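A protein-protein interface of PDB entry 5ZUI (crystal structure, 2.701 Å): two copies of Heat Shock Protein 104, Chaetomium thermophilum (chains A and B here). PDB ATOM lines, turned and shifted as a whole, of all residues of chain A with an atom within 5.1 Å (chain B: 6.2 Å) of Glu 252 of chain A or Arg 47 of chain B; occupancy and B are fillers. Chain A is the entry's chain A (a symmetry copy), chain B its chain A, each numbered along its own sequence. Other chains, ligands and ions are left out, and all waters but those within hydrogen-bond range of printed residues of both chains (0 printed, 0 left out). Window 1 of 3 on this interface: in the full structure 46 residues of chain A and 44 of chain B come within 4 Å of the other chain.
The side-chain carboxylate (OE2) of Glu 40 of chain B lies within salt-bridge range of the guanidinium group (NH2) of Arg 43 of chain B (2.9 Å).
The backbone carbonyl oxygen of Ile 46 of chain B sits at hydrogen-bond distance from the side-chain hydroxyl of Ser 50 of chain B, 2.9 Å away.
Of the 12 printed residues of chain B, 5 touch a printed residue of chain A.
Printed residues of chain B that touch a printed residue of chain A: Glu 40, Arg 44, Ile 46, Arg 47 and Arg 51.
Hydrophobic or aromatic side chains of chain A within 4 Å of the printed part of chain B: Ala 255 and Val 259.
Among the printed residues, 8 pairs touch across the chains.
NH1 of Arg 47 of chain B lies within salt-bridge range of OE2 of Glu 252 of chain A.
NH2 of Arg 51 of chain B lies within salt-bridge range of OD1 of Asp 251 of chain A, at 2.6 Å.
NH2 of Arg 51 of chain B lies within salt-bridge range of OE1 of Glu 252 of chain A (3.3 Å).
The guanidinium group (NH2) of Arg 410 of chain A sits close to the guanidinium group (NH1) of Arg 44 of chain B (3.1 Å).
Of the printed residues of chain B, Glu 252 of chain A touches Arg 47 (2.6 Å) and Arg 51 (3.3 Å).
Of chain A, only Glu 252 and Ala 255 come within 4 Å of Arg 47 of chain B.
Printed residues of chain B within 4 Å of Ala 255 of chain A: Arg 47 and Arg 51.
Of the printed residues of chain B, Asp 251 of chain A touches Arg 51.
Printed residues of chain B within 4 Å of Arg 410 of chain A: Glu 40 and Arg 44.
Printed residues of chain B within 4 Å of Val 259 of chain A: Ile 46.
Asp 248 of chain A touches none of the printed residues of chain B.
The nearest residue of chain A that does not touch Arg 47 of chain B is Ala 256 of chain A (4.1 Å).
No position is printed for both chains.
Among the printed residues, pairs that only touch across the chains: Ala 255 of chain A with Arg 51 of chain B, Ala 255 of chain A with Arg 47 of chain B, Arg 410 of chain A with Glu 40 of chain B and Val 259 of chain A with Ile 46 of chain B.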
ATOM      1  N   VAL A 247      25.141  17.179  11.284  1.00  0.00           N
ATOM      2  CA  VAL A 247      23.977  16.301  11.344  1.00  0.00           C
ATOM      3  C   VAL A 247      23.349  16.343  12.734  1.00  0.00           C
ATOM      4  O   VAL A 247      22.135  16.529  12.875  1.00  0.00           O
ATOM      5  CB  VAL A 247      24.356  14.866  10.931  1.00  0.00           C
ATOM      6  CG1 VAL A 247      23.289  13.869  11.378  1.00  0.00           C
ATOM      7  CG2 VAL A 247      24.554  14.784   9.426  1.00  0.00           C
ATOM      8  N   ASP A 248      24.169  16.178  13.781  1.00  0.00           N
ATOM      9  CA  ASP A 248      23.655  16.265  15.148  1.00  0.00           C
ATOM     10  C   ASP A 248      22.980  17.602  15.407  1.00  0.00           C
ATOM     11  O   ASP A 248      22.010  17.672  16.170  1.00  0.00           O
ATOM     12  CB  ASP A 248      24.782  16.055  16.162  1.00  0.00           C
ATOM     13  CG  ASP A 248      25.052  14.588  16.447  1.00  0.00           C
ATOM     14  OD1 ASP A 248      24.635  13.729  15.637  1.00  0.00           O
ATOM     15  OD2 ASP A 248      25.688  14.294  17.482  1.00  0.00           O
ATOM     16  N   LEU A 249      23.470  18.667  14.769  1.00  0.00           N
ATOM     17  CA  LEU A 249      22.934  20.003  15.003  1.00  0.00           C
ATOM     18  C   LEU A 249      21.548  20.159  14.384  1.00  0.00           C
ATOM     19  O   LEU A 249      20.626  20.676  15.025  1.00  0.00           O
ATOM     20  CB  LEU A 249      23.910  21.041  14.451  1.00  0.00           C
ATOM     21  CG  LEU A 249      23.541  22.517  14.365  1.00  0.00           C
ATOM     22  CD1 LEU A 249      22.982  23.024  15.684  1.00  0.00           C
ATOM     23  CD2 LEU A 249      24.781  23.299  13.968  1.00  0.00           C
ATOM     24  N   ILE A 250      21.377  19.710  13.139  1.00  0.00           N
ATOM     25  CA  ILE A 250      20.064  19.776  12.504  1.00  0.00           C
ATOM     26  C   ILE A 250      19.092  18.817  13.182  1.00  0.00           C
ATOM     27  O   ILE A 250      17.909  19.131  13.361  1.00  0.00           O
ATOM     28  CB  ILE A 250      20.189  19.496  10.995  1.00  0.00           C
ATOM     29  CG1 ILE A 250      20.445  20.794  10.229  1.00  0.00           C
ATOM     30  CG2 ILE A 250      18.946  18.816  10.458  1.00  0.00           C
ATOM     31  CD1 ILE A 250      20.760  20.574   8.772  1.00  0.00           C
ATOM     32  N   ASP A 251      19.575  17.638  13.581  1.00  0.00           N
ATOM     33  CA  ASP A 251      18.701  16.667  14.231  1.00  0.00           C
ATOM     34  C   ASP A 251      18.182  17.190  15.566  1.00  0.00           C
ATOM     35  O   ASP A 251      17.041  16.899  15.945  1.00  0.00           O
ATOM     36  CB  ASP A 251      19.445  15.342  14.416  1.00  0.00           C
ATOM     37  CG  ASP A 251      18.604  14.285  15.111  1.00  0.00           C
ATOM     38  OD1 ASP A 251      18.713  14.151  16.350  1.00  0.00           O
ATOM     39  OD2 ASP A 251      17.839  13.580  14.415  1.00  0.00           O
ATOM     40  N   GLU A 252      18.998  17.967  16.285  1.00  0.00           N
ATOM     41  CA  GLU A 252      18.558  18.525  17.557  1.00  0.00           C
ATOM     42  C   GLU A 252      17.600  19.691  17.342  1.00  0.00           C
ATOM     43  O   GLU A 252      16.630  19.847  18.094  1.00  0.00           O
ATOM     44  CB  GLU A 252      19.769  18.958  18.391  1.00  0.00           C
ATOM     45  CG  GLU A 252      19.440  19.381  19.816  1.00  0.00           C
ATOM     46  CD  GLU A 252      18.945  18.228  20.679  1.00  0.00           C
ATOM     47  OE1 GLU A 252      19.067  17.058  20.252  1.00  0.00           O
ATOM     48  OE2 GLU A 252      18.435  18.494  21.791  1.00  0.00           O
ATOM     49  N   ALA A 253      17.853  20.509  16.317  1.00  0.00           N
ATOM     50  CA  ALA A 253      16.915  21.568  15.968  1.00  0.00           C
ATOM     51  C   ALA A 253      15.566  20.991  15.563  1.00  0.00           C
ATOM     52  O   ALA A 253      14.515  21.474  16.006  1.00  0.00           O
ATOM     53  CB  ALA A 253      17.486  22.428  14.842  1.00  0.00           C
ATOM     54  N   ALA A 254      15.576  19.958  14.717  1.00  0.00           N
ATOM     55  CA  ALA A 254      14.329  19.321  14.312  1.00  0.00           C
ATOM     56  C   ALA A 254      13.563  18.797  15.517  1.00  0.00           C
ATOM     57  O   ALA A 254      12.350  19.002  15.629  1.00  0.00           O
ATOM     58  CB  ALA A 254      14.613  18.192  13.321  1.00  0.00           C
ATOM     59  N   ALA A 255      14.258  18.127  16.439  1.00  0.00           N
ATOM     60  CA  ALA A 255      13.594  17.622  17.633  1.00  0.00           C
ATOM     61  C   ALA A 255      13.069  18.758  18.499  1.00  0.00           C
ATOM     62  O   ALA A 255      12.063  18.586  19.198  1.00  0.00           O
ATOM     63  CB  ALA A 255      14.545  16.732  18.433  1.00  0.00           C
ATOM     64  N   ALA A 256      13.726  19.920  18.464  1.00  0.00           N
ATOM     65  CA  ALA A 256      13.244  21.066  19.229  1.00  0.00           C
ATOM     66  C   ALA A 256      11.981  21.652  18.617  1.00  0.00           C
ATOM     67  O   ALA A 256      11.174  22.266  19.323  1.00  0.00           O
ATOM     68  CB  ALA A 256      14.330  22.138  19.325  1.00  0.00           C
ATOM     69  N   VAL A 259       8.562  19.441  19.188  1.00  0.00           N
ATOM     70  CA  VAL A 259       7.760  19.758  20.367  1.00  0.00           C
ATOM     71  C   VAL A 259       7.085  21.127  20.252  1.00  0.00           C
ATOM     72  O   VAL A 259       5.981  21.317  20.774  1.00  0.00           O
ATOM     73  CB  VAL A 259       8.634  19.666  21.631  1.00  0.00           C
ATOM     74  CG1 VAL A 259       9.936  20.393  21.412  1.00  0.00           C
ATOM     75  CG2 VAL A 259       7.907  20.234  22.846  1.00  0.00           C
ATOM     76  N   ILE A 407      20.212  26.624  19.010  1.00  0.00           N
ATOM     77  CA  ILE A 407      20.715  25.341  19.491  1.00  0.00           C
ATOM     78  C   ILE A 407      22.216  25.422  19.741  1.00  0.00           C
ATOM     79  O   ILE A 407      22.714  24.985  20.784  1.00  0.00           O
ATOM     80  CB  ILE A 407      20.367  24.213  18.500  1.00  0.00           C
ATOM     81  CG1 ILE A 407      18.868  23.899  18.533  1.00  0.00           C
ATOM     82  CG2 ILE A 407      21.153  22.955  18.840  1.00  0.00           C
ATOM     83  CD1 ILE A 407      18.391  23.270  19.823  1.00  0.00           C
ATOM     84  N   ARG A 410      23.129  27.418  22.981  1.00  0.00           N
ATOM     85  CA  ARG A 410      22.999  26.633  24.206  1.00  0.00           C
ATOM     86  C   ARG A 410      24.199  25.707  24.393  1.00  0.00           C
ATOM     87  O   ARG A 410      24.770  25.626  25.487  1.00  0.00           O
ATOM     88  CB  ARG A 410      21.687  25.840  24.180  1.00  0.00           C
ATOM     89  CG  ARG A 410      21.675  24.590  25.052  1.00  0.00           C
ATOM     90  CD  ARG A 410      20.480  23.688  24.736  1.00  0.00           C
ATOM     91  NE  ARG A 410      20.876  22.291  24.554  1.00  0.00           N
ATOM     92  CZ  ARG A 410      21.107  21.429  25.543  1.00  0.00           C
ATOM     93  NH1 ARG A 410      20.982  21.804  26.812  1.00  0.00           N
ATOM     94  NH2 ARG A 410      21.465  20.185  25.256  1.00  0.00           N
ATOM     95  N   TRP A 411      24.607  25.011  23.328  1.00  0.00           N
ATOM     96  CA  TRP A 411      25.755  24.111  23.413  1.00  0.00           C
ATOM     97  C   TRP A 411      27.052  24.881  23.620  1.00  0.00           C
ATOM     98  O   TRP A 411      27.856  24.540  24.496  1.00  0.00           O
ATOM     99  CB  TRP A 411      25.857  23.259  22.146  1.00  0.00           C
ATOM    100  CG  TRP A 411      24.770  22.242  21.964  1.00  0.00           C
ATOM    101  CD1 TRP A 411      23.788  21.911  22.852  1.00  0.00           C
ATOM    102  CD2 TRP A 411      24.561  21.421  20.810  1.00  0.00           C
ATOM    103  NE1 TRP A 411      22.977  20.935  22.321  1.00  0.00           N
ATOM    104  CE2 TRP A 411      23.433  20.617  21.068  1.00  0.00           C
ATOM    105  CE3 TRP A 411      25.220  21.287  19.583  1.00  0.00           C
ATOM    106  CZ2 TRP A 411      22.949  19.690  20.143  1.00  0.00           C
ATOM    107  CZ3 TRP A 411      24.737  20.369  18.665  1.00  0.00           C
ATOM    108  CH2 TRP A 411      23.613  19.583  18.951  1.00  0.00           C
ATOM    109  N   GLU B  40      16.273  24.535  31.697  1.00  0.00           N
ATOM    110  CA  GLU B  40      16.858  23.909  30.516  1.00  0.00           C
ATOM    111  C   GLU B  40      16.904  22.392  30.647  1.00  0.00           C
ATOM    112  O   GLU B  40      16.762  21.684  29.643  1.00  0.00           O
ATOM    113  CB  GLU B  40      18.256  24.469  30.248  1.00  0.00           C
ATOM    114  CG  GLU B  40      18.800  24.121  28.852  1.00  0.00           C
ATOM    115  CD  GLU B  40      18.385  25.121  27.773  1.00  0.00           C
ATOM    116  OE1 GLU B  40      18.974  26.225  27.722  1.00  0.00           O
ATOM    117  OE2 GLU B  40      17.477  24.800  26.972  1.00  0.00           O
ATOM    118  N   ILE B  42      14.642  20.568  32.267  1.00  0.00           N
ATOM    119  CA  ILE B  42      13.287  20.065  32.064  1.00  0.00           C
ATOM    120  C   ILE B  42      12.889  20.176  30.595  1.00  0.00           C
ATOM    121  O   ILE B  42      12.150  19.327  30.075  1.00  0.00           O
ATOM    122  CB  ILE B  42      12.297  20.798  32.988  1.00  0.00           C
ATOM    123  CG1 ILE B  42      12.666  20.551  34.455  1.00  0.00           C
ATOM    124  CG2 ILE B  42      10.871  20.334  32.720  1.00  0.00           C
ATOM    125  CD1 ILE B  42      11.921  21.447  35.446  1.00  0.00           C
ATOM    126  N   ARG B  43      13.380  21.198  29.891  1.00  0.00           N
ATOM    127  CA  ARG B  43      13.146  21.249  28.453  1.00  0.00           C
ATOM    128  C   ARG B  43      13.800  20.063  27.762  1.00  0.00           C
ATOM    129  O   ARG B  43      13.204  19.449  26.869  1.00  0.00           O
ATOM    130  CB  ARG B  43      13.652  22.570  27.876  1.00  0.00           C
ATOM    131  CG  ARG B  43      12.604  23.683  27.912  1.00  0.00           C
ATOM    132  CD  ARG B  43      12.938  24.796  26.938  1.00  0.00           C
ATOM    133  NE  ARG B  43      14.255  25.364  27.203  1.00  0.00           N
ATOM    134  CZ  ARG B  43      14.497  26.273  28.142  1.00  0.00           C
ATOM    135  NH1 ARG B  43      13.509  26.718  28.908  1.00  0.00           N
ATOM    136  NH2 ARG B  43      15.729  26.737  28.318  1.00  0.00           N
ATOM    137  N   ARG B  44      15.019  19.707  28.186  1.00  0.00           N
ATOM    138  CA  ARG B  44      15.701  18.559  27.597  1.00  0.00           C
ATOM    139  C   ARG B  44      14.913  17.276  27.818  1.00  0.00           C
ATOM    140  O   ARG B  44      14.786  16.454  26.904  1.00  0.00           O
ATOM    141  CB  ARG B  44      17.106  18.427  28.178  1.00  0.00           C
ATOM    142  CG  ARG B  44      18.072  19.475  27.675  1.00  0.00           C
ATOM    143  CD  ARG B  44      18.616  19.103  26.309  1.00  0.00           C
ATOM    144  NE  ARG B  44      19.114  17.729  26.269  1.00  0.00           N
ATOM    145  CZ  ARG B  44      20.236  17.317  26.854  1.00  0.00           C
ATOM    146  NH1 ARG B  44      20.993  18.172  27.533  1.00  0.00           N
ATOM    147  NH2 ARG B  44      20.603  16.046  26.754  1.00  0.00           N
ATOM    148  N   VAL B  45      14.367  17.090  29.021  1.00  0.00           N
ATOM    149  CA  VAL B  45      13.591  15.885  29.303  1.00  0.00           C
ATOM    150  C   VAL B  45      12.354  15.839  28.424  1.00  0.00           C
ATOM    151  O   VAL B  45      12.018  14.793  27.850  1.00  0.00           O
ATOM    152  CB  VAL B  45      13.226  15.822  30.799  1.00  0.00           C
ATOM    153  CG1 VAL B  45      12.021  14.915  31.021  1.00  0.00           C
ATOM    154  CG2 VAL B  45      14.424  15.348  31.627  1.00  0.00           C
ATOM    155  N   ILE B  46      11.659  16.976  28.307  1.00  0.00           N
ATOM    156  CA  ILE B  46      10.490  17.079  27.438  1.00  0.00           C
ATOM    157  C   ILE B  46      10.882  16.793  25.995  1.00  0.00           C
ATOM    158  O   ILE B  46      10.216  16.024  25.290  1.00  0.00           O
ATOM    159  CB  ILE B  46       9.848  18.471  27.585  1.00  0.00           C
ATOM    160  CG1 ILE B  46       9.063  18.561  28.895  1.00  0.00           C
ATOM    161  CG2 ILE B  46       8.964  18.806  26.381  1.00  0.00           C
ATOM    162  CD1 ILE B  46       8.759  19.973  29.316  1.00  0.00           C
ATOM    163  N   ARG B  47      11.984  17.400  25.544  1.00  0.00           N
ATOM    164  CA  ARG B  47      12.427  17.198  24.171  1.00  0.00           C
ATOM    165  C   ARG B  47      12.749  15.731  23.905  1.00  0.00           C
ATOM    166  O   ARG B  47      12.334  15.176  22.883  1.00  0.00           O
ATOM    167  CB  ARG B  47      13.637  18.085  23.879  1.00  0.00           C
ATOM    168  CG  ARG B  47      13.969  18.187  22.408  1.00  0.00           C
ATOM    169  CD  ARG B  47      15.196  19.053  22.177  1.00  0.00           C
ATOM    170  NE  ARG B  47      15.152  20.301  22.937  1.00  0.00           N
ATOM    171  CZ  ARG B  47      16.218  20.894  23.465  1.00  0.00           C
ATOM    172  NH1 ARG B  47      17.422  20.353  23.322  1.00  0.00           N
ATOM    173  NH2 ARG B  47      16.085  22.029  24.142  1.00  0.00           N
ATOM    174  N   ILE B  48      13.475  15.084  24.822  1.00  0.00           N
ATOM    175  CA  ILE B  48      13.816  13.675  24.642  1.00  0.00           C
ATOM    176  C   ILE B  48      12.551  12.829  24.602  1.00  0.00           C
ATOM    177  O   ILE B  48      12.370  11.996  23.706  1.00  0.00           O
ATOM    178  CB  ILE B  48      14.771  13.200  25.752  1.00  0.00           C
ATOM    179  CG1 ILE B  48      16.152  13.829  25.586  1.00  0.00           C
ATOM    180  CG2 ILE B  48      14.868  11.679  25.760  1.00  0.00           C
ATOM    181  CD1 ILE B  48      17.103  13.460  26.681  1.00  0.00           C
ATOM    182  N   LEU B  49      11.652  13.036  25.570  1.00  0.00           N
ATOM    183  CA  LEU B  49      10.420  12.252  25.623  1.00  0.00           C
ATOM    184  C   LEU B  49       9.597  12.401  24.348  1.00  0.00           C
ATOM    185  O   LEU B  49       8.931  11.449  23.924  1.00  0.00           O
ATOM    186  CB  LEU B  49       9.589  12.667  26.839  1.00  0.00           C
ATOM    187  CG  LEU B  49      10.073  12.231  28.222  1.00  0.00           C
ATOM    188  CD1 LEU B  49       9.272  12.927  29.290  1.00  0.00           C
ATOM    189  CD2 LEU B  49       9.952  10.729  28.382  1.00  0.00           C
ATOM    190  N   SER B  50       9.639  13.578  23.721  1.00  0.00           N
ATOM    191  CA  SER B  50       8.848  13.839  22.527  1.00  0.00           C
ATOM    192  C   SER B  50       9.445  13.218  21.274  1.00  0.00           C
ATOM    193  O   SER B  50       8.747  13.104  20.262  1.00  0.00           O
ATOM    194  CB  SER B  50       8.688  15.346  22.323  1.00  0.00           C
ATOM    195  OG  SER B  50       7.960  15.928  23.392  1.00  0.00           O
ATOM    196  N   ARG B  51      10.713  12.824  21.314  1.00  0.00           N
ATOM    197  CA  ARG B  51      11.308  12.125  20.187  1.00  0.00           C
ATOM    198  C   ARG B  51      10.583  10.809  19.931  1.00  0.00           C
ATOM    199  O   ARG B  51       9.898  10.262  20.799  1.00  0.00           O
ATOM    200  CB  ARG B  51      12.789  11.850  20.450  1.00  0.00           C
ATOM    201  CG  ARG B  51      13.685  13.065  20.306  1.00  0.00           C
ATOM    202  CD  ARG B  51      15.145  12.678  20.406  1.00  0.00           C
ATOM    203  NE  ARG B  51      16.023  13.760  19.971  1.00  0.00           N
ATOM    204  CZ  ARG B  51      16.693  13.767  18.821  1.00  0.00           C
ATOM    205  NH1 ARG B  51      16.589  12.742  17.980  1.00  0.00           N
ATOM    206  NH2 ARG B  51      17.471  14.799  18.514  1.00  0.00           N
ATOM    207  N   GLN B 190      18.953   8.686  26.557  1.00  0.00           N
ATOM    208  CA  GLN B 190      19.783   9.824  26.180  1.00  0.00           C
ATOM    209  C   GLN B 190      20.212  10.535  27.452  1.00  0.00           C
ATOM    210  O   GLN B 190      19.366  10.917  28.268  1.00  0.00           O
ATOM    211  CB  GLN B 190      19.038  10.779  25.241  1.00  0.00           C
ATOM    212  CG  GLN B 190      19.931  11.466  24.209  1.00  0.00           C
ATOM    213  CD  GLN B 190      19.144  12.070  23.048  1.00  0.00           C
ATOM    214  OE1 GLN B 190      18.102  11.545  22.635  1.00  0.00           O
ATOM    215  NE2 GLN B 190      19.643  13.181  22.514  1.00  0.00           N
